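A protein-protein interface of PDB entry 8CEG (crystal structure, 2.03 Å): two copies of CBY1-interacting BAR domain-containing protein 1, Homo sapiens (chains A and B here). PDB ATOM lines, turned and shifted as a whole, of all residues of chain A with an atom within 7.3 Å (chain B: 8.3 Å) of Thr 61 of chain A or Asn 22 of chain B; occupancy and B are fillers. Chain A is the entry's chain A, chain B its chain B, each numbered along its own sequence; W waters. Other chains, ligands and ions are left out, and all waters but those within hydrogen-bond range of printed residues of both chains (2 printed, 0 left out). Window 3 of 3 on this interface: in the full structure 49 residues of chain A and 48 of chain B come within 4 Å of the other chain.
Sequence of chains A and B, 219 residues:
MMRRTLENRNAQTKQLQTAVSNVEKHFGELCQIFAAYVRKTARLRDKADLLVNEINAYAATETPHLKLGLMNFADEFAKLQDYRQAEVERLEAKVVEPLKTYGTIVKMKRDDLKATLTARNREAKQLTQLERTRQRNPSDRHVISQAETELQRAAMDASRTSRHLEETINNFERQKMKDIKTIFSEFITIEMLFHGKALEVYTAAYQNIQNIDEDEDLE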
ATOM      1  N   GLU A  54     -17.961  -8.514 -26.630  1.00  0.00           N
ATOM      2  CA  GLU A  54     -17.700  -9.835 -26.047  1.00  0.00           C
ATOM      3  C   GLU A  54     -16.315 -10.379 -26.410  1.00  0.00           C
ATOM      4  O   GLU A  54     -15.666 -11.007 -25.573  1.00  0.00           O
ATOM      5  CB  GLU A  54     -18.789 -10.812 -26.468  1.00  0.00           C
ATOM      6  CG  GLU A  54     -18.561 -12.219 -26.002  1.00  0.00           C
ATOM      7  CD  GLU A  54     -18.386 -12.348 -24.514  1.00  0.00           C
ATOM      8  OE1 GLU A  54     -19.065 -11.604 -23.768  1.00  0.00           O
ATOM      9  OE2 GLU A  54     -17.579 -13.222 -24.102  1.00  0.00           O
ATOM     10  N   ILE A  55     -15.832 -10.137 -27.628  1.00  0.00           N
ATOM     11  CA  ILE A  55     -14.473 -10.554 -27.993  1.00  0.00           C
ATOM     12  C   ILE A  55     -13.446  -9.899 -27.086  1.00  0.00           C
ATOM     13  O   ILE A  55     -12.484 -10.537 -26.640  1.00  0.00           O
ATOM     14  CB  ILE A  55     -14.214 -10.219 -29.473  1.00  0.00           C
ATOM     15  CG1 ILE A  55     -15.131 -11.083 -30.355  1.00  0.00           C
ATOM     16  CG2 ILE A  55     -12.780 -10.396 -29.861  1.00  0.00           C
ATOM     17  CD1 ILE A  55     -15.193 -10.597 -31.777  1.00  0.00           C
ATOM     18  N   ASN A  56     -13.609  -8.599 -26.830  1.00  0.00           N
ATOM     19  CA  ASN A  56     -12.705  -7.901 -25.918  1.00  0.00           C
ATOM     20  C   ASN A  56     -12.849  -8.398 -24.483  1.00  0.00           C
ATOM     21  O   ASN A  56     -11.856  -8.508 -23.754  1.00  0.00           O
ATOM     22  CB  ASN A  56     -12.974  -6.398 -25.987  1.00  0.00           C
ATOM     23  CG  ASN A  56     -12.329  -5.765 -27.176  1.00  0.00           C
ATOM     24  OD1 ASN A  56     -11.200  -6.102 -27.555  1.00  0.00           O
ATOM     25  ND2 ASN A  56     -13.037  -4.862 -27.786  1.00  0.00           N
ATOM     26  N   ALA A  57     -14.074  -8.650 -24.034  1.00  0.00           N
ATOM     27  CA  ALA A  57     -14.280  -9.197 -22.692  1.00  0.00           C
ATOM     28  C   ALA A  57     -13.665 -10.594 -22.551  1.00  0.00           C
ATOM     29  O   ALA A  57     -13.058 -10.920 -21.513  1.00  0.00           O
ATOM     30  CB  ALA A  57     -15.780  -9.204 -22.397  1.00  0.00           C
ATOM     31  N   TYR A  58     -13.781 -11.436 -23.579  1.00  0.00           N
ATOM     32  CA  TYR A  58     -13.119 -12.742 -23.496  1.00  0.00           C
ATOM     33  C   TYR A  58     -11.611 -12.593 -23.625  1.00  0.00           C
ATOM     34  O   TYR A  58     -10.853 -13.277 -22.928  1.00  0.00           O
ATOM     35  CB  TYR A  58     -13.653 -13.697 -24.564  1.00  0.00           C
ATOM     36  CG  TYR A  58     -12.823 -14.974 -24.735  1.00  0.00           C
ATOM     37  CD1 TYR A  58     -12.527 -15.797 -23.661  1.00  0.00           C
ATOM     38  CD2 TYR A  58     -12.335 -15.342 -25.987  1.00  0.00           C
ATOM     39  CE1 TYR A  58     -11.754 -16.980 -23.829  1.00  0.00           C
ATOM     40  CE2 TYR A  58     -11.548 -16.501 -26.166  1.00  0.00           C
ATOM     41  CZ  TYR A  58     -11.275 -17.318 -25.089  1.00  0.00           C
ATOM     42  OH  TYR A  58     -10.516 -18.455 -25.283  1.00  0.00           O
ATOM     43  N   ALA A  59     -11.151 -11.717 -24.528  1.00  0.00           N
ATOM     44  CA  ALA A  59      -9.717 -11.528 -24.690  1.00  0.00           C
ATOM     45  C   ALA A  59      -9.064 -11.138 -23.372  1.00  0.00           C
ATOM     46  O   ALA A  59      -7.930 -11.536 -23.091  1.00  0.00           O
ATOM     47  CB  ALA A  59      -9.423 -10.454 -25.724  1.00  0.00           C
ATOM     48  N   ALA A  60      -9.746 -10.289 -22.593  1.00  0.00           N
ATOM     49  CA  ALA A  60      -9.188  -9.798 -21.341  1.00  0.00           C
ATOM     50  C   ALA A  60      -8.788 -10.941 -20.403  1.00  0.00           C
ATOM     51  O   ALA A  60      -7.863 -10.788 -19.595  1.00  0.00           O
ATOM     52  CB  ALA A  60     -10.209  -8.842 -20.702  1.00  0.00           C
ATOM     53  N   THR A  61      -9.453 -12.091 -20.502  1.00  0.00           N
ATOM     54  CA  THR A  61      -9.209 -13.224 -19.633  1.00  0.00           C
ATOM     55  C   THR A  61      -8.117 -14.151 -20.139  1.00  0.00           C
ATOM     56  O   THR A  61      -7.887 -15.170 -19.513  1.00  0.00           O
ATOM     57  CB  THR A  61     -10.480 -14.069 -19.473  1.00  0.00           C
ATOM     58  OG1 THR A  61     -10.757 -14.726 -20.726  1.00  0.00           O
ATOM     59  CG2 THR A  61     -11.681 -13.208 -19.107  1.00  0.00           C
ATOM     60  N   GLU A  62      -7.471 -13.871 -21.262  1.00  0.00           N
ATOM     61  CA  GLU A  62      -6.718 -14.914 -21.945  1.00  0.00           C
ATOM     62  C   GLU A  62      -5.219 -14.657 -21.880  1.00  0.00           C
ATOM     63  O   GLU A  62      -4.741 -13.683 -21.272  1.00  0.00           O
ATOM     64  CB  GLU A  62      -7.194 -15.056 -23.396  1.00  0.00           C
ATOM     65  CG  GLU A  62      -8.328 -16.074 -23.576  1.00  0.00           C
ATOM     66  CD  GLU A  62      -7.893 -17.522 -23.240  1.00  0.00           C
ATOM     67  OE1 GLU A  62      -6.712 -17.729 -22.957  1.00  0.00           O
ATOM     68  OE2 GLU A  62      -8.724 -18.455 -23.234  1.00  0.00           O
ATOM     69  N   THR A  63      -4.468 -15.589 -22.497  1.00  0.00           N
ATOM     70  CA  THR A  63      -3.011 -15.488 -22.495  1.00  0.00           C
ATOM     71  C   THR A  63      -2.574 -14.428 -23.505  1.00  0.00           C
ATOM     72  O   THR A  63      -3.303 -14.138 -24.453  1.00  0.00           O
ATOM     73  CB  THR A  63      -2.372 -16.837 -22.830  1.00  0.00           C
ATOM     74  OG1 THR A  63      -2.898 -17.326 -24.080  1.00  0.00           O
ATOM     75  CG2 THR A  63      -2.671 -17.868 -21.724  1.00  0.00           C
ATOM     76  N   LYS A  67      -4.882 -12.991 -26.300  1.00  0.00           N
ATOM     77  CA  LYS A  67      -5.532 -11.734 -25.945  1.00  0.00           C
ATOM     78  C   LYS A  67      -5.248 -10.645 -26.983  1.00  0.00           C
ATOM     79  O   LYS A  67      -6.159  -9.937 -27.437  1.00  0.00           O
ATOM     80  CB  LYS A  67      -5.109 -11.308 -24.546  1.00  0.00           C
ATOM     81  CG  LYS A  67      -5.380  -9.846 -24.239  1.00  0.00           C
ATOM     82  CD  LYS A  67      -5.198  -9.464 -22.753  1.00  0.00           C
ATOM     83  CE  LYS A  67      -4.026 -10.046 -22.069  1.00  0.00           C
ATOM     84  NZ  LYS A  67      -2.808  -9.214 -22.259  1.00  0.00           N
ATOM     85  N   GLN B  15      -7.108 -25.198 -11.483  1.00  0.00           N
ATOM     86  CA  GLN B  15      -6.800 -24.638 -12.796  1.00  0.00           C
ATOM     87  C   GLN B  15      -7.797 -25.092 -13.872  1.00  0.00           C
ATOM     88  O   GLN B  15      -8.208 -24.286 -14.727  1.00  0.00           O
ATOM     89  CB  GLN B  15      -5.381 -25.006 -13.202  1.00  0.00           C
ATOM     90  CG  GLN B  15      -5.003 -24.550 -14.601  1.00  0.00           C
ATOM     91  CD  GLN B  15      -3.563 -24.893 -14.936  1.00  0.00           C
ATOM     92  OE1 GLN B  15      -2.956 -25.730 -14.281  1.00  0.00           O
ATOM     93  NE2 GLN B  15      -3.021 -24.259 -15.976  1.00  0.00           N
ATOM     94  N   LEU B  16      -8.164 -26.380 -13.879  1.00  0.00           N
ATOM     95  CA  LEU B  16      -9.067 -26.885 -14.904  1.00  0.00           C
ATOM     96  C   LEU B  16     -10.467 -26.295 -14.743  1.00  0.00           C
ATOM     97  O   LEU B  16     -11.063 -25.805 -15.717  1.00  0.00           O
ATOM     98  CB  LEU B  16      -9.104 -28.418 -14.885  1.00  0.00           C
ATOM     99  CG  LEU B  16      -9.908 -29.185 -15.952  1.00  0.00           C
ATOM    100  CD1 LEU B  16      -9.573 -28.786 -17.394  1.00  0.00           C
ATOM    101  CD2 LEU B  16      -9.682 -30.686 -15.748  1.00  0.00           C
ATOM    102  N   GLN B  17     -11.002 -26.314 -13.525  1.00  0.00           N
ATOM    103  CA  GLN B  17     -12.344 -25.777 -13.301  1.00  0.00           C
ATOM    104  C   GLN B  17     -12.442 -24.288 -13.662  1.00  0.00           C
ATOM    105  O   GLN B  17     -13.503 -23.813 -14.094  1.00  0.00           O
ATOM    106  CB  GLN B  17     -12.736 -26.023 -11.837  1.00  0.00           C
ATOM    107  CG  GLN B  17     -14.202 -25.704 -11.471  1.00  0.00           C
ATOM    108  CD  GLN B  17     -15.196 -26.805 -11.857  1.00  0.00           C
ATOM    109  OE1 GLN B  17     -14.977 -27.986 -11.580  1.00  0.00           O
ATOM    110  NE2 GLN B  17     -16.304 -26.412 -12.481  1.00  0.00           N
ATOM    111  N   THR B  18     -11.386 -23.514 -13.417  1.00  0.00           N
ATOM    112  CA  THR B  18     -11.436 -22.092 -13.751  1.00  0.00           C
ATOM    113  C   THR B  18     -11.459 -21.899 -15.251  1.00  0.00           C
ATOM    114  O   THR B  18     -12.284 -21.134 -15.767  1.00  0.00           O
ATOM    115  CB  THR B  18     -10.256 -21.371 -13.113  1.00  0.00           C
ATOM    116  OG1 THR B  18     -10.476 -21.342 -11.703  1.00  0.00           O
ATOM    117  CG2 THR B  18     -10.076 -19.957 -13.626  1.00  0.00           C
ATOM    118  N   ALA B  19     -10.615 -22.654 -15.967  1.00  0.00           N
ATOM    119  CA  ALA B  19     -10.593 -22.583 -17.421  1.00  0.00           C
ATOM    120  C   ALA B  19     -11.900 -23.059 -18.026  1.00  0.00           C
ATOM    121  O   ALA B  19     -12.415 -22.425 -18.960  1.00  0.00           O
ATOM    122  CB  ALA B  19      -9.434 -23.391 -17.986  1.00  0.00           C
ATOM    123  N   VAL B  20     -12.444 -24.181 -17.533  1.00  0.00           N
ATOM    124  CA  VAL B  20     -13.681 -24.729 -18.093  1.00  0.00           C
ATOM    125  C   VAL B  20     -14.823 -23.729 -17.926  1.00  0.00           C
ATOM    126  O   VAL B  20     -15.651 -23.548 -18.828  1.00  0.00           O
ATOM    127  CB  VAL B  20     -14.027 -26.077 -17.430  1.00  0.00           C
ATOM    128  CG1 VAL B  20     -15.530 -26.386 -17.626  1.00  0.00           C
ATOM    129  CG2 VAL B  20     -13.169 -27.191 -18.003  1.00  0.00           C
ATOM    130  N   SER B  21     -14.859 -23.038 -16.783  1.00  0.00           N
ATOM    131  CA  SER B  21     -15.915 -22.077 -16.509  1.00  0.00           C
ATOM    132  C   SER B  21     -15.769 -20.839 -17.395  1.00  0.00           C
ATOM    133  O   SER B  21     -16.770 -20.253 -17.839  1.00  0.00           O
ATOM    134  CB  SER B  21     -15.863 -21.674 -15.039  1.00  0.00           C
ATOM    135  OG  SER B  21     -16.547 -22.613 -14.245  1.00  0.00           O
ATOM    136  N   ASN B  22     -14.520 -20.416 -17.615  1.00  0.00           N
ATOM    137  CA  ASN B  22     -14.229 -19.294 -18.494  1.00  0.00           C
ATOM    138  C   ASN B  22     -14.639 -19.591 -19.923  1.00  0.00           C
ATOM    139  O   ASN B  22     -15.274 -18.760 -20.590  1.00  0.00           O
ATOM    140  CB  ASN B  22     -12.739 -18.963 -18.428  1.00  0.00           C
ATOM    141  CG  ASN B  22     -12.436 -17.605 -19.027  1.00  0.00           C
ATOM    142  OD1 ASN B  22     -13.016 -16.622 -18.596  1.00  0.00           O
ATOM    143  ND2 ASN B  22     -11.526 -17.541 -20.013  1.00  0.00           N
ATOM    144  N   VAL B  23     -14.235 -20.750 -20.439  1.00  0.00           N
ATOM    145  CA  VAL B  23     -14.641 -21.125 -21.795  1.00  0.00           C
ATOM    146  C   VAL B  23     -16.164 -21.203 -21.887  1.00  0.00           C
ATOM    147  O   VAL B  23     -16.775 -20.671 -22.822  1.00  0.00           O
ATOM    148  CB  VAL B  23     -13.948 -22.435 -22.222  1.00  0.00           C
ATOM    149  CG1 VAL B  23     -14.698 -23.129 -23.372  1.00  0.00           C
ATOM    150  CG2 VAL B  23     -12.501 -22.138 -22.657  1.00  0.00           C
ATOM    151  N   GLU B  24     -16.806 -21.822 -20.902  1.00  0.00           N
ATOM    152  CA  GLU B  24     -18.249 -21.937 -20.917  1.00  0.00           C
ATOM    153  C   GLU B  24     -18.908 -20.578 -21.023  1.00  0.00           C
ATOM    154  O   GLU B  24     -19.804 -20.379 -21.844  1.00  0.00           O
ATOM    155  CB  GLU B  24     -18.778 -22.629 -19.670  1.00  0.00           C
ATOM    156  CG  GLU B  24     -20.266 -22.375 -19.492  1.00  0.00           C
ATOM    157  CD  GLU B  24     -20.898 -23.249 -18.457  1.00  0.00           C
ATOM    158  OE1 GLU B  24     -20.653 -23.011 -17.243  1.00  0.00           O
ATOM    159  OE2 GLU B  24     -21.640 -24.191 -18.847  1.00  0.00           O
ATOM    160  N   LYS B  25     -18.511 -19.651 -20.153  1.00  0.00           N
ATOM    161  CA  LYS B  25     -19.158 -18.343 -20.098  1.00  0.00           C
ATOM    162  C   LYS B  25     -18.988 -17.568 -21.413  1.00  0.00           C
ATOM    163  O   LYS B  25     -19.964 -17.089 -22.002  1.00  0.00           O
ATOM    164  CB  LYS B  25     -18.594 -17.578 -18.907  1.00  0.00           C
ATOM    165  CG  LYS B  25     -18.901 -16.118 -18.922  1.00  0.00           C
ATOM    166  CD  LYS B  25     -18.535 -15.472 -17.586  1.00  0.00           C
ATOM    167  CE  LYS B  25     -19.040 -14.006 -17.572  1.00  0.00           C
ATOM    168  NZ  LYS B  25     -18.844 -13.321 -16.254  1.00  0.00           N
ATOM    169  N   HIS B  26     -17.753 -17.485 -21.910  1.00  0.00           N
ATOM    170  CA  HIS B  26     -17.431 -16.669 -23.063  1.00  0.00           C
ATOM    171  C   HIS B  26     -17.730 -17.355 -24.385  1.00  0.00           C
ATOM    172  O   HIS B  26     -18.218 -16.696 -25.305  1.00  0.00           O
ATOM    173  CB  HIS B  26     -15.965 -16.246 -22.991  1.00  0.00           C
ATOM    174  CG  HIS B  26     -15.713 -15.268 -21.884  1.00  0.00           C
ATOM    175  ND1 HIS B  26     -16.181 -13.969 -21.928  1.00  0.00           N
ATOM    176  CD2 HIS B  26     -15.134 -15.418 -20.666  1.00  0.00           C
ATOM    177  CE1 HIS B  26     -15.867 -13.351 -20.800  1.00  0.00           C
ATOM    178  NE2 HIS B  26     -15.216 -14.201 -20.027  1.00  0.00           N
ATOM    179  N   PHE B  27     -17.449 -18.654 -24.535  1.00  0.00           N
ATOM    180  CA  PHE B  27     -17.859 -19.319 -25.768  1.00  0.00           C
ATOM    181  C   PHE B  27     -19.377 -19.325 -25.908  1.00  0.00           C
ATOM    182  O   PHE B  27     -19.899 -19.296 -27.028  1.00  0.00           O
ATOM    183  CB  PHE B  27     -17.334 -20.748 -25.848  1.00  0.00           C
ATOM    184  CG  PHE B  27     -15.914 -20.855 -26.300  1.00  0.00           C
ATOM    185  CD1 PHE B  27     -14.953 -19.952 -25.858  1.00  0.00           C
ATOM    186  CD2 PHE B  27     -15.529 -21.878 -27.128  1.00  0.00           C
ATOM    187  CE1 PHE B  27     -13.621 -20.068 -26.267  1.00  0.00           C
ATOM    188  CE2 PHE B  27     -14.192 -22.007 -27.541  1.00  0.00           C
ATOM    189  CZ  PHE B  27     -13.241 -21.120 -27.100  1.00  0.00           C
ATOM    190  N   GLY B  28     -20.093 -19.458 -24.784  1.00  0.00           N
ATOM    191  CA  GLY B  28     -21.546 -19.448 -24.823  1.00  0.00           C
ATOM    192  C   GLY B  28     -22.089 -18.076 -25.188  1.00  0.00           C
ATOM    193  O   GLY B  28     -23.078 -17.957 -25.915  1.00  0.00           O
ATOM    194  N   GLU B  29     -21.436 -17.022 -24.706  1.00  0.00           N
ATOM    195  CA  GLU B  29     -21.825 -15.668 -25.092  1.00  0.00           C
ATOM    196  C   GLU B  29     -21.528 -15.408 -26.573  1.00  0.00           C
ATOM    197  O   GLU B  29     -22.372 -14.871 -27.289  1.00  0.00           O
ATOM    198  CB  GLU B  29     -21.106 -14.665 -24.196  1.00  0.00           C
ATOM    199  CG  GLU B  29     -21.668 -13.255 -24.284  1.00  0.00           C
ATOM    200  CD  GLU B  29     -23.121 -13.165 -23.795  1.00  0.00           C
ATOM    201  OE1 GLU B  29     -23.530 -14.014 -22.960  1.00  0.00           O
ATOM    202  OE2 GLU B  29     -23.848 -12.258 -24.257  1.00  0.00           O
ATOM    203  N   VAL B 106     -17.817 -28.697 -22.488  1.00  0.00           N
ATOM    204  CA  VAL B 106     -17.818 -28.195 -21.121  1.00  0.00           C
ATOM    205  C   VAL B 106     -18.594 -29.118 -20.194  1.00  0.00           C
ATOM    206  O   VAL B 106     -18.170 -29.377 -19.058  1.00  0.00           O
ATOM    207  CB  VAL B 106     -18.384 -26.755 -21.122  1.00  0.00           C
ATOM    208  CG1 VAL B 106     -18.952 -26.377 -19.756  1.00  0.00           C
ATOM    209  CG2 VAL B 106     -17.286 -25.775 -21.584  1.00  0.00           C
ATOM    210  N   ARG B 110     -17.101 -31.016 -16.833  1.00  0.00           N
ATOM    211  CA  ARG B 110     -17.663 -30.887 -15.493  1.00  0.00           C
ATOM    212  C   ARG B 110     -18.086 -32.224 -14.895  1.00  0.00           C
ATOM    213  O   ARG B 110     -17.923 -32.429 -13.690  1.00  0.00           O
ATOM    214  CB  ARG B 110     -18.803 -29.881 -15.500  1.00  0.00           C
ATOM    215  CG  ARG B 110     -18.245 -28.495 -15.581  1.00  0.00           C
ATOM    216  CD  ARG B 110     -19.194 -27.507 -14.961  1.00  0.00           C
ATOM    217  NE  ARG B 110     -18.627 -26.161 -14.927  1.00  0.00           N
ATOM    218  CZ  ARG B 110     -19.136 -25.125 -15.585  1.00  0.00           C
ATOM    219  NH1 ARG B 110     -20.195 -25.263 -16.375  1.00  0.00           N
ATOM    220  NH2 ARG B 110     -18.574 -23.925 -15.449  1.00  0.00           N
ATOM    221  N   PHE B 172      -7.211 -29.675 -23.344  1.00  0.00           N
ATOM    222  CA  PHE B 172      -8.331 -28.743 -23.421  1.00  0.00           C
ATOM    223  C   PHE B 172      -7.875 -27.396 -23.967  1.00  0.00           C
ATOM    224  O   PHE B 172      -8.547 -26.807 -24.825  1.00  0.00           O
ATOM    225  CB  PHE B 172      -8.984 -28.602 -22.044  1.00  0.00           C
ATOM    226  CG  PHE B 172     -10.161 -27.653 -22.008  1.00  0.00           C
ATOM    227  CD1 PHE B 172     -11.397 -28.041 -22.504  1.00  0.00           C
ATOM    228  CD2 PHE B 172     -10.042 -26.386 -21.448  1.00  0.00           C
ATOM    229  CE1 PHE B 172     -12.503 -27.180 -22.468  1.00  0.00           C
ATOM    230  CE2 PHE B 172     -11.149 -25.518 -21.407  1.00  0.00           C
ATOM    231  CZ  PHE B 172     -12.379 -25.925 -21.921  1.00  0.00           C
ATOM    232  N   GLU B 173      -6.712 -26.914 -23.492  1.00  0.00           N
ATOM    233  CA  GLU B 173      -6.197 -25.604 -23.862  1.00  0.00           C
ATOM    234  C   GLU B 173      -5.665 -25.609 -25.283  1.00  0.00           C
ATOM    235  O   GLU B 173      -5.889 -24.653 -26.042  1.00  0.00           O
ATOM    236  CB  GLU B 173      -5.104 -25.166 -22.872  1.00  0.00           C
ATOM    237  CG  GLU B 173      -5.647 -24.994 -21.448  1.00  0.00           C
ATOM    238  CD  GLU B 173      -6.551 -23.751 -21.246  1.00  0.00           C
ATOM    239  OE1 GLU B 173      -6.695 -22.918 -22.178  1.00  0.00           O
ATOM    240  OE2 GLU B 173      -7.155 -23.634 -20.146  1.00  0.00           O
ATOM    241  N   LYS B 176      -8.766 -25.688 -27.388  1.00  0.00           N
ATOM    242  CA  LYS B 176      -9.474 -24.424 -27.288  1.00  0.00           C
ATOM    243  C   LYS B 176      -8.842 -23.377 -28.206  1.00  0.00           C
ATOM    244  O   LYS B 176      -9.547 -22.640 -28.921  1.00  0.00           O
ATOM    245  CB  LYS B 176      -9.466 -23.959 -25.822  1.00  0.00           C
ATOM    246  CG  LYS B 176      -9.921 -22.493 -25.598  1.00  0.00           C
ATOM    247  CD  LYS B 176      -9.300 -21.868 -24.348  1.00  0.00           C
ATOM    248  CE  LYS B 176      -7.853 -21.421 -24.618  1.00  0.00           C
ATOM    249  NZ  LYS B 176      -7.249 -20.647 -23.500  1.00  0.00           N
HETATM  250  O   HOH W   1     -10.060 -19.510 -21.223  1.00  0.00           O
HETATM  251  O   HOH W   2      -4.604 -20.002 -24.089  1.00  0.00           O
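OG1 of Thr 61 of chain A lies within hydrogen-bond range of ND2 of Asn 22 of chain B.
OE2 of Glu 62 of chain A is in salt-bridge range of NZ of Lys 176 of chain B (2.7 Å).
The side-chain carboxylate (OE2) of Glu 54 of chain A lies within hydrogen-bond range of a ring nitrogen (ND1) of His 26 of chain B, at 2.7 Å.
Water W1 bridges OE2 of Glu 62 of chain A (2.6 Å) and ND2 of Asn 22 of chain B (2.7 Å).
Water W2 lies within hydrogen-bond range of the side-chain amino group (NZ) of Lys 176 of chain B (2.8 Å), the side-chain hydroxyl (OG1) of Thr 63 of chain A (3.2 Å) and the side-chain carboxylate (OE1) of Glu 62 of chain A (3.3 Å).
Of the printed residues of chain B, Glu 54 of chain A touches His 26 and Glu 29.
Of the printed residues of chain B, Ala 57 of chain A touches His 26 (3.8 Å).
No residue of chain B comes within 4 Å of Ala 60 of chain A.
Thr 61 of chain A touches two residues of chain B.
Of chain A, only Tyr 58 and Thr 61 come within 4 Å of Asn 22 of chain B.
Printed residues of chain A within 4 Å of His 26 of chain B: Glu 54 (2.7 Å), Ala 57 (3.8 Å), Tyr 58 (3.5 Å) and Thr 61 (3.8 Å).
Printed residues of chain A within 4 Å of Lys 176 of chain B: Tyr 58 (3.7 Å) and Glu 62 (2.7 Å).
The nearest printed residue of chain A that does not touch Glu 29 of chain B is Ala 57 of chain A (7.4 Å).
Glu 54 of chain A touches Glu 29 of chain B.
O of Ala 57 of chain A touches CE1 of His 26 of chain B, at 3.8 Å.
Asn 22 of chain B touches Tyr 58 of chain A (ND2 to CE1, 3.9 Å).
Tyr 58 of chain A touches His 26 of chain B (CD1 to CB, 3.5 Å).
Tyr 58 of chain A touches Phe 27 of chain B (OH to CE1, 3.6 Å).
Tyr 58 of chain A touches Lys 176 of chain B.
CG2 of Thr 61 of chain A touches NE2 of His 26 of chain B (3.8 Å).
No position is printed for both chains.
The side-chain carboxylate (OE1) of Glu 173 of chain B is in salt-bridge range of the side-chain amino group (NZ) of Lys 176 of chain B, at 2.7 Å.
The side-chain hydroxyl (OG1) of Thr 61 of chain A sits at hydrogen-bond distance from the backbone carbonyl oxygen (O) of Tyr 58 of chain A, at 2.6 Å.
OH of Tyr 58 of chain A lies within hydrogen-bond range of OE2 of Glu 62 of chain A (2.7 Å).
Of the 20 printed residues of chain B, 5 touch a printed residue of chain A.
Printed residues of chain B that touch a printed residue of chain A: Asn 22, His 26, Phe 27, Glu 29 and Lys 176.
Hydrophobic or aromatic side chains of chain B within 4 Å of the printed part of chain A: His 26 and Phe 27.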
